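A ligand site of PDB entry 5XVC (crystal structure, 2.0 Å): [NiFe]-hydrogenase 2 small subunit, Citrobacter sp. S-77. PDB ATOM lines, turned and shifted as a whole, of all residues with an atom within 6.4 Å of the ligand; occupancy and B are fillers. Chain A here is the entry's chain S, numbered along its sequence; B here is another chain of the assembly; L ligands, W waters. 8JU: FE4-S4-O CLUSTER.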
ATOM      1  N   GLN A  20      19.784   8.115  21.429  1.00  0.00           N
ATOM      2  CA  GLN A  20      18.672   7.434  20.766  1.00  0.00           C
ATOM      3  C   GLN A  20      18.946   7.404  19.273  1.00  0.00           C
ATOM      4  O   GLN A  20      18.387   8.199  18.520  1.00  0.00           O
ATOM      5  CB  GLN A  20      17.341   8.117  21.060  1.00  0.00           C
ATOM      6  CG  GLN A  20      16.761   7.842  22.441  1.00  0.00           C
ATOM      7  CD  GLN A  20      15.497   8.641  22.693  1.00  0.00           C
ATOM      8  OE1 GLN A  20      15.511   9.875  22.619  1.00  0.00           O
ATOM      9  NE2 GLN A  20      14.377   7.947  22.988  1.00  0.00           N
ATOM     10  N   GLU A  21      19.795   6.479  18.840  1.00  0.00           N
ATOM     11  CA  GLU A  21      20.254   6.420  17.454  1.00  0.00           C
ATOM     12  C   GLU A  21      19.743   5.142  16.773  1.00  0.00           C
ATOM     13  O   GLU A  21      19.306   4.220  17.452  1.00  0.00           O
ATOM     14  CB  GLU A  21      21.786   6.505  17.392  1.00  0.00           C
ATOM     15  CG  GLU A  21      22.533   5.159  17.242  1.00  0.00           C
ATOM     16  CD  GLU A  21      22.640   4.366  18.528  1.00  0.00           C
ATOM     17  OE1 GLU A  21      23.663   4.495  19.244  1.00  0.00           O
ATOM     18  OE2 GLU A  21      21.711   3.572  18.824  1.00  0.00           O
ATOM     19  N   CYS A  22      19.800   5.104  15.442  1.00  0.00           N
ATOM     20  CA  CYS A  22      19.452   3.897  14.682  1.00  0.00           C
ATOM     21  C   CYS A  22      20.705   3.262  14.086  1.00  0.00           C
ATOM     22  O   CYS A  22      20.641   2.200  13.455  1.00  0.00           O
ATOM     23  CB  CYS A  22      18.431   4.203  13.566  1.00  0.00           C
ATOM     24  SG  CYS A  22      19.137   4.735  11.937  1.00  0.00           S
ATOM     25  N   THR A  23      21.831   3.949  14.275  1.00  0.00           N
ATOM     26  CA  THR A  23      23.168   3.542  13.820  1.00  0.00           C
ATOM     27  C   THR A  23      23.442   3.825  12.330  1.00  0.00           C
ATOM     28  O   THR A  23      24.556   3.606  11.827  1.00  0.00           O
ATOM     29  CB  THR A  23      23.510   2.087  14.250  1.00  0.00           C
ATOM     30  OG1 THR A  23      23.090   1.895  15.609  1.00  0.00           O
ATOM     31  CG2 THR A  23      25.012   1.815  14.171  1.00  0.00           C
ATOM     32  N   GLY A  24      22.435   4.347  11.635  1.00  0.00           N
ATOM     33  CA  GLY A  24      22.621   4.839  10.275  1.00  0.00           C
ATOM     34  C   GLY A  24      23.754   5.834  10.109  1.00  0.00           C
ATOM     35  O   GLY A  24      24.420   5.864   9.084  1.00  0.00           O
ATOM     36  N   CYS A  25      23.984   6.669  11.124  1.00  0.00           N
ATOM     37  CA  CYS A  25      25.013   7.705  11.036  1.00  0.00           C
ATOM     38  C   CYS A  25      26.418   7.094  11.096  1.00  0.00           C
ATOM     39  O   CYS A  25      27.308   7.500  10.367  1.00  0.00           O
ATOM     40  CB  CYS A  25      24.811   8.782  12.127  1.00  0.00           C
ATOM     41  SG  CYS A  25      23.388   9.880  11.862  1.00  0.00           S
ATOM     42  N   THR A  26      26.610   6.106  11.975  1.00  0.00           N
ATOM     43  CA  THR A  26      27.849   5.334  11.977  1.00  0.00           C
ATOM     44  C   THR A  26      27.968   4.544  10.677  1.00  0.00           C
ATOM     45  O   THR A  26      29.045   4.478  10.086  1.00  0.00           O
ATOM     46  CB  THR A  26      27.913   4.390  13.193  1.00  0.00           C
ATOM     47  OG1 THR A  26      28.015   5.181  14.376  1.00  0.00           O
ATOM     48  CG2 THR A  26      29.128   3.468  13.111  1.00  0.00           C
ATOM     49  N   ASP A  81      25.478  11.082  18.484  1.00  0.00           N
ATOM     50  CA  ASP A  81      24.641  10.478  17.467  1.00  0.00           C
ATOM     51  C   ASP A  81      23.322  10.085  18.147  1.00  0.00           C
ATOM     52  O   ASP A  81      23.312   9.287  19.078  1.00  0.00           O
ATOM     53  CB  ASP A  81      25.338   9.219  16.925  1.00  0.00           C
ATOM     54  CG  ASP A  81      24.598   8.617  15.772  1.00  0.00           C
ATOM     55  OD1 ASP A  81      23.658   9.286  15.335  1.00  0.00           O
ATOM     56  OD2 ASP A  81      24.930   7.501  15.310  1.00  0.00           O
ATOM     57  N   GLY A  82      22.215  10.666  17.682  1.00  0.00           N
ATOM     58  CA  GLY A  82      20.924  10.336  18.245  1.00  0.00           C
ATOM     59  C   GLY A  82      20.285  11.426  19.104  1.00  0.00           C
ATOM     60  O   GLY A  82      20.959  12.326  19.589  1.00  0.00           O
ATOM     61  N   SER A  83      18.985  11.331  19.286  1.00  0.00           N
ATOM     62  CA  SER A  83      18.274  12.278  20.133  1.00  0.00           C
ATOM     63  C   SER A  83      18.476  11.879  21.598  1.00  0.00           C
ATOM     64  O   SER A  83      18.924  10.767  21.894  1.00  0.00           O
ATOM     65  CB  SER A  83      16.797  12.301  19.787  1.00  0.00           C
ATOM     66  OG  SER A  83      16.192  11.048  20.026  1.00  0.00           O
ATOM     67  N   ILE A 117      25.773  14.795  14.873  1.00  0.00           N
ATOM     68  CA  ILE A 117      25.635  14.205  13.548  1.00  0.00           C
ATOM     69  C   ILE A 117      24.258  13.578  13.389  1.00  0.00           C
ATOM     70  O   ILE A 117      23.782  12.865  14.274  1.00  0.00           O
ATOM     71  CB  ILE A 117      26.737  13.165  13.274  1.00  0.00           C
ATOM     72  CG1 ILE A 117      26.698  12.734  11.808  1.00  0.00           C
ATOM     73  CG2 ILE A 117      26.627  11.952  14.232  1.00  0.00           C
ATOM     74  CD1 ILE A 117      27.721  11.628  11.494  1.00  0.00           C
ATOM     75  N   GLY A 118      23.594  13.859  12.276  1.00  0.00           N
ATOM     76  CA  GLY A 118      22.280  13.332  12.014  1.00  0.00           C
ATOM     77  C   GLY A 118      21.211  14.246  12.550  1.00  0.00           C
ATOM     78  O   GLY A 118      21.425  14.984  13.521  1.00  0.00           O
ATOM     79  N   SER A 119      20.051  14.208  11.911  1.00  0.00           N
ATOM     80  CA  SER A 119      18.934  15.060  12.287  1.00  0.00           C
ATOM     81  C   SER A 119      18.455  14.843  13.726  1.00  0.00           C
ATOM     82  O   SER A 119      17.913  15.774  14.340  1.00  0.00           O
ATOM     83  CB  SER A 119      17.769  14.864  11.302  1.00  0.00           C
ATOM     84  OG  SER A 119      18.134  15.298  10.004  1.00  0.00           O
ATOM     85  N   CYS A 120      18.623  13.622  14.243  1.00  0.00           N
ATOM     86  CA  CYS A 120      18.144  13.342  15.599  1.00  0.00           C
ATOM     87  C   CYS A 120      18.881  14.191  16.613  1.00  0.00           C
ATOM     88  O   CYS A 120      18.265  14.828  17.454  1.00  0.00           O
ATOM     89  CB  CYS A 120      18.290  11.874  15.962  1.00  0.00           C
ATOM     90  SG  CYS A 120      17.243  10.853  14.958  1.00  0.00           S
ATOM     91  N   ALA A 121      20.196  14.190  16.513  1.00  0.00           N
ATOM     92  CA  ALA A 121      20.995  14.947  17.464  1.00  0.00           C
ATOM     93  C   ALA A 121      20.952  16.438  17.151  1.00  0.00           C
ATOM     94  O   ALA A 121      21.199  17.280  18.018  1.00  0.00           O
ATOM     95  CB  ALA A 121      22.410  14.427  17.495  1.00  0.00           C
ATOM     96  N   GLY A 125      14.811  15.041  15.398  1.00  0.00           N
ATOM     97  CA  GLY A 125      14.612  14.080  14.319  1.00  0.00           C
ATOM     98  C   GLY A 125      13.425  13.134  14.497  1.00  0.00           C
ATOM     99  O   GLY A 125      12.421  13.492  15.129  1.00  0.00           O
ATOM    100  N   VAL A 126      13.548  11.936  13.934  1.00  0.00           N
ATOM    101  CA  VAL A 126      12.422  11.022  13.866  1.00  0.00           C
ATOM    102  C   VAL A 126      11.920  10.631  15.250  1.00  0.00           C
ATOM    103  O   VAL A 126      10.706  10.488  15.479  1.00  0.00           O
ATOM    104  CB  VAL A 126      12.748   9.758  13.026  1.00  0.00           C
ATOM    105  CG1 VAL A 126      13.870   8.928  13.679  1.00  0.00           C
ATOM    106  CG2 VAL A 126      11.503   8.919  12.824  1.00  0.00           C
ATOM    107  N   GLY A 153      20.462  15.407   8.624  1.00  0.00           N
ATOM    108  CA  GLY A 153      20.203  14.456   7.566  1.00  0.00           C
ATOM    109  C   GLY A 153      20.024  13.078   8.181  1.00  0.00           C
ATOM    110  O   GLY A 153      20.437  12.858   9.303  1.00  0.00           O
ATOM    111  N   CYS A 154      19.419  12.157   7.452  1.00  0.00           N
ATOM    112  CA  CYS A 154      19.049  10.918   8.111  1.00  0.00           C
ATOM    113  C   CYS A 154      19.387   9.675   7.293  1.00  0.00           C
ATOM    114  O   CYS A 154      18.476   9.024   6.759  1.00  0.00           O
ATOM    115  CB  CYS A 154      17.558  10.977   8.475  1.00  0.00           C
ATOM    116  SG  CYS A 154      16.971   9.617   9.534  1.00  0.00           S
ATOM    117  N   PRO A 155      20.693   9.342   7.181  1.00  0.00           N
ATOM    118  CA  PRO A 155      21.819  10.114   7.739  1.00  0.00           C
ATOM    119  C   PRO A 155      22.341  11.082   6.694  1.00  0.00           C
ATOM    120  O   PRO A 155      21.988  10.954   5.509  1.00  0.00           O
ATOM    121  CB  PRO A 155      22.871   9.032   7.993  1.00  0.00           C
ATOM    122  CG  PRO A 155      22.668   8.078   6.847  1.00  0.00           C
ATOM    123  CD  PRO A 155      21.139   8.048   6.644  1.00  0.00           C
ATOM    124  N   PRO A 156      23.171  12.048   7.118  1.00  0.00           N
ATOM    125  CA  PRO A 156      23.818  12.909   6.123  1.00  0.00           C
ATOM    126  C   PRO A 156      24.840  12.148   5.292  1.00  0.00           C
ATOM    127  O   PRO A 156      25.276  11.067   5.704  1.00  0.00           O
ATOM    128  CB  PRO A 156      24.540  13.960   6.982  1.00  0.00           C
ATOM    129  CG  PRO A 156      24.776  13.279   8.286  1.00  0.00           C
ATOM    130  CD  PRO A 156      23.550  12.415   8.502  1.00  0.00           C
ATOM    131  N   PHE A 265       9.667  13.690   8.595  1.00  0.00           N
ATOM    132  CA  PHE A 265       9.008  13.006   9.722  1.00  0.00           C
ATOM    133  C   PHE A 265       7.834  13.778  10.321  1.00  0.00           C
ATOM    134  O   PHE A 265       7.266  13.355  11.320  1.00  0.00           O
ATOM    135  CB  PHE A 265      10.043  12.575  10.778  1.00  0.00           C
ATOM    136  CG  PHE A 265      11.287  11.969  10.186  1.00  0.00           C
ATOM    137  CD1 PHE A 265      11.251  10.712   9.594  1.00  0.00           C
ATOM    138  CD2 PHE A 265      12.482  12.685  10.165  1.00  0.00           C
ATOM    139  CE1 PHE A 265      12.403  10.165   9.022  1.00  0.00           C
ATOM    140  CE2 PHE A 265      13.629  12.136   9.601  1.00  0.00           C
ATOM    141  CZ  PHE A 265      13.597  10.881   9.023  1.00  0.00           C
ATOM    142  N   ARG B  39      12.496   4.099  21.811  1.00  0.00           N
ATOM    143  CA  ARG B  39      12.113   5.289  21.081  1.00  0.00           C
ATOM    144  C   ARG B  39      10.610   5.445  20.893  1.00  0.00           C
ATOM    145  O   ARG B  39      10.131   6.564  20.753  1.00  0.00           O
ATOM    146  CB  ARG B  39      12.822   5.314  19.725  1.00  0.00           C
ATOM    147  CG  ARG B  39      14.281   5.764  19.817  1.00  0.00           C
ATOM    148  CD  ARG B  39      14.986   5.619  18.482  1.00  0.00           C
ATOM    149  NE  ARG B  39      15.046   4.215  18.096  1.00  0.00           N
ATOM    150  CZ  ARG B  39      15.300   3.770  16.878  1.00  0.00           C
ATOM    151  NH1 ARG B  39      15.546   4.627  15.875  1.00  0.00           N
ATOM    152  NH2 ARG B  39      15.324   2.467  16.659  1.00  0.00           N
ATOM    153  N   ARG B  59      13.509   4.046   9.887  1.00  0.00           N
ATOM    154  CA  ARG B  59      14.430   4.548  10.902  1.00  0.00           C
ATOM    155  C   ARG B  59      14.443   3.718  12.205  1.00  0.00           C
ATOM    156  O   ARG B  59      15.073   4.109  13.199  1.00  0.00           O
ATOM    157  CB  ARG B  59      14.155   6.023  11.203  1.00  0.00           C
ATOM    158  CG  ARG B  59      14.832   7.001  10.228  1.00  0.00           C
ATOM    159  CD  ARG B  59      14.354   6.854   8.781  1.00  0.00           C
ATOM    160  NE  ARG B  59      15.158   7.665   7.851  1.00  0.00           N
ATOM    161  CZ  ARG B  59      14.921   7.792   6.547  1.00  0.00           C
ATOM    162  NH1 ARG B  59      13.878   7.186   6.001  1.00  0.00           N
ATOM    163  NH2 ARG B  59      15.728   8.540   5.794  1.00  0.00           N
ATOM    164  N   CYS B  61      16.017   1.040  12.246  1.00  0.00           N
ATOM    165  CA  CYS B  61      17.417   0.678  12.234  1.00  0.00           C
ATOM    166  C   CYS B  61      18.138   1.014  10.931  1.00  0.00           C
ATOM    167  O   CYS B  61      17.608   0.806   9.838  1.00  0.00           O
ATOM    168  CB  CYS B  61      17.566  -0.802  12.562  1.00  0.00           C
ATOM    169  SG  CYS B  61      19.279  -1.262  12.751  1.00  0.00           S
ATOM    170  N   GLY B  62      19.357   1.508  11.053  1.00  0.00           N
ATOM    171  CA  GLY B  62      20.176   1.841   9.882  1.00  0.00           C
ATOM    172  C   GLY B  62      21.231   0.792   9.540  1.00  0.00           C
ATOM    173  O   GLY B  62      21.925   0.925   8.531  1.00  0.00           O
ATOM    174  N   PRO B 213      22.957   4.657   3.945  1.00  0.00           N
ATOM    175  CA  PRO B 213      21.779   4.118   4.670  1.00  0.00           C
ATOM    176  C   PRO B 213      20.458   4.800   4.307  1.00  0.00           C
ATOM    177  O   PRO B 213      20.454   5.951   3.844  1.00  0.00           O
ATOM    178  CB  PRO B 213      22.113   4.375   6.140  1.00  0.00           C
ATOM    179  CG  PRO B 213      23.620   4.495   6.189  1.00  0.00           C
ATOM    180  CD  PRO B 213      23.991   5.161   4.865  1.00  0.00           C
ATOM    181  N   HIS B 214      19.368   4.039   4.474  1.00  0.00           N
ATOM    182  CA  HIS B 214      18.001   4.490   4.265  1.00  0.00           C
ATOM    183  C   HIS B 214      17.632   4.752   2.804  1.00  0.00           C
ATOM    184  O   HIS B 214      17.820   5.850   2.288  1.00  0.00           O
ATOM    185  CB  HIS B 214      17.672   5.669   5.183  1.00  0.00           C
ATOM    186  CG  HIS B 214      17.711   5.306   6.630  1.00  0.00           C
ATOM    187  ND1 HIS B 214      17.517   4.009   7.070  1.00  0.00           N
ATOM    188  CD2 HIS B 214      17.977   6.047   7.736  1.00  0.00           C
ATOM    189  CE1 HIS B 214      17.631   3.968   8.388  1.00  0.00           C
ATOM    190  NE2 HIS B 214      17.915   5.195   8.810  1.00  0.00           N
HETATM  191  S2  8JU L   1      17.757   8.004  12.865  1.00  0.00           S
HETATM  192 FE2  8JU L   1      18.889   9.858  13.664  1.00  0.00          FE
HETATM  193 FE3  8JU L   1      18.568   9.120  11.076  1.00  0.00          FE
HETATM  194  S3  8JU L   1      19.392  11.118  11.948  1.00  0.00           S
HETATM  195 FE1  8JU L   1      19.652   6.943  12.235  1.00  0.00          FE
HETATM  196  S4  8JU L   1      20.234   7.792  10.299  1.00  0.00           S
HETATM  197  S1  8JU L   1      21.475   6.915  13.528  1.00  0.00           S
HETATM  198 FE4  8JU L   1      22.009   9.040  13.845  1.00  0.00          FE
HETATM  199  O   8JU L   1      20.332   9.801  14.458  1.00  0.00           O
HETATM  200  O   HOH W   1      21.467  11.984  15.323  1.00  0.00           O
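The side-chain carboxylate (OD1) of Asp 81 binds an iron atom (FE4) of the ligand.
SG of Cys 154 binds FE3 of the ligand (2.3 Å).
The backbone NH (N) of Cys 22 lies close to a sulfur (S1) of the ligand (3.1 Å).
SG of Cys 22 is bound to FE1 of the ligand (2.3 Å).
The backbone NH (N) of Cys 120 lies close to a sulfur (S3) of the ligand (3.5 Å).
An iron atom (FE2) of the ligand is bound by the side-chain sulfur (SG) of Cys 120 (2.3 Å).
N of Cys 25 sits close to S1 of the ligand (3.5 Å).
The side-chain sulfur of Cys 25 binds an iron atom (FE4) of the ligand (2.6 Å).
The backbone NH (N) of Thr 23 lies close to a sulfur (S1) of the ligand (3.1 Å).
A sulfur (S3) of the ligand lies close to the backbone NH (N) of Ser 119, at 3.2 Å.
The backbone NH of Gly 24 sits close to a sulfur (S1) of the ligand, at 3.3 Å.
A ring nitrogen (NE2) of His 214 of chain B lies close to a sulfur (S4) of the ligand (3.8 Å).
O of Cys 154 lies within hydrogen-bond range of NH2 of Arg 59 of chain B (3.0 Å).
The side-chain sulfur (SG) of Cys 22 lies close to the backbone NH (N) of Gly 24.
The side-chain sulfur (SG) of Cys 22 lies close to a ring nitrogen (NE2) of His 214 of chain B, at 3.4 Å.
O of Cys 22 sits at hydrogen-bond distance from N of Gly 62 of chain B (2.8 Å).
SG of Cys 61 of chain B sits close to O of Cys 22 (3.8 Å).
The side-chain hydroxyl of Ser 119 is in hydrogen-bond range of the backbone NH of Gly 153 (2.7 Å).
The backbone carbonyl oxygen of Ser 119 sits at hydrogen-bond distance from the backbone NH of Gly 125 (3.4 Å).
O of Gly 153 lies close to S3 of the ligand, at 3.3 Å.
A sulfur (S4) of the ligand sits close to the backbone nitrogen of Pro 155 (3.5 Å).
Residues that only touch the ligand: Gly 118, Gly 82 and Glu 21.
Hydrophobic or aromatic side chains within 4 Å of the ligand: Pro 155 and His 214 of chain B.
Along chain A the residues within 4 Å of the ligand span positions 21 to 155.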
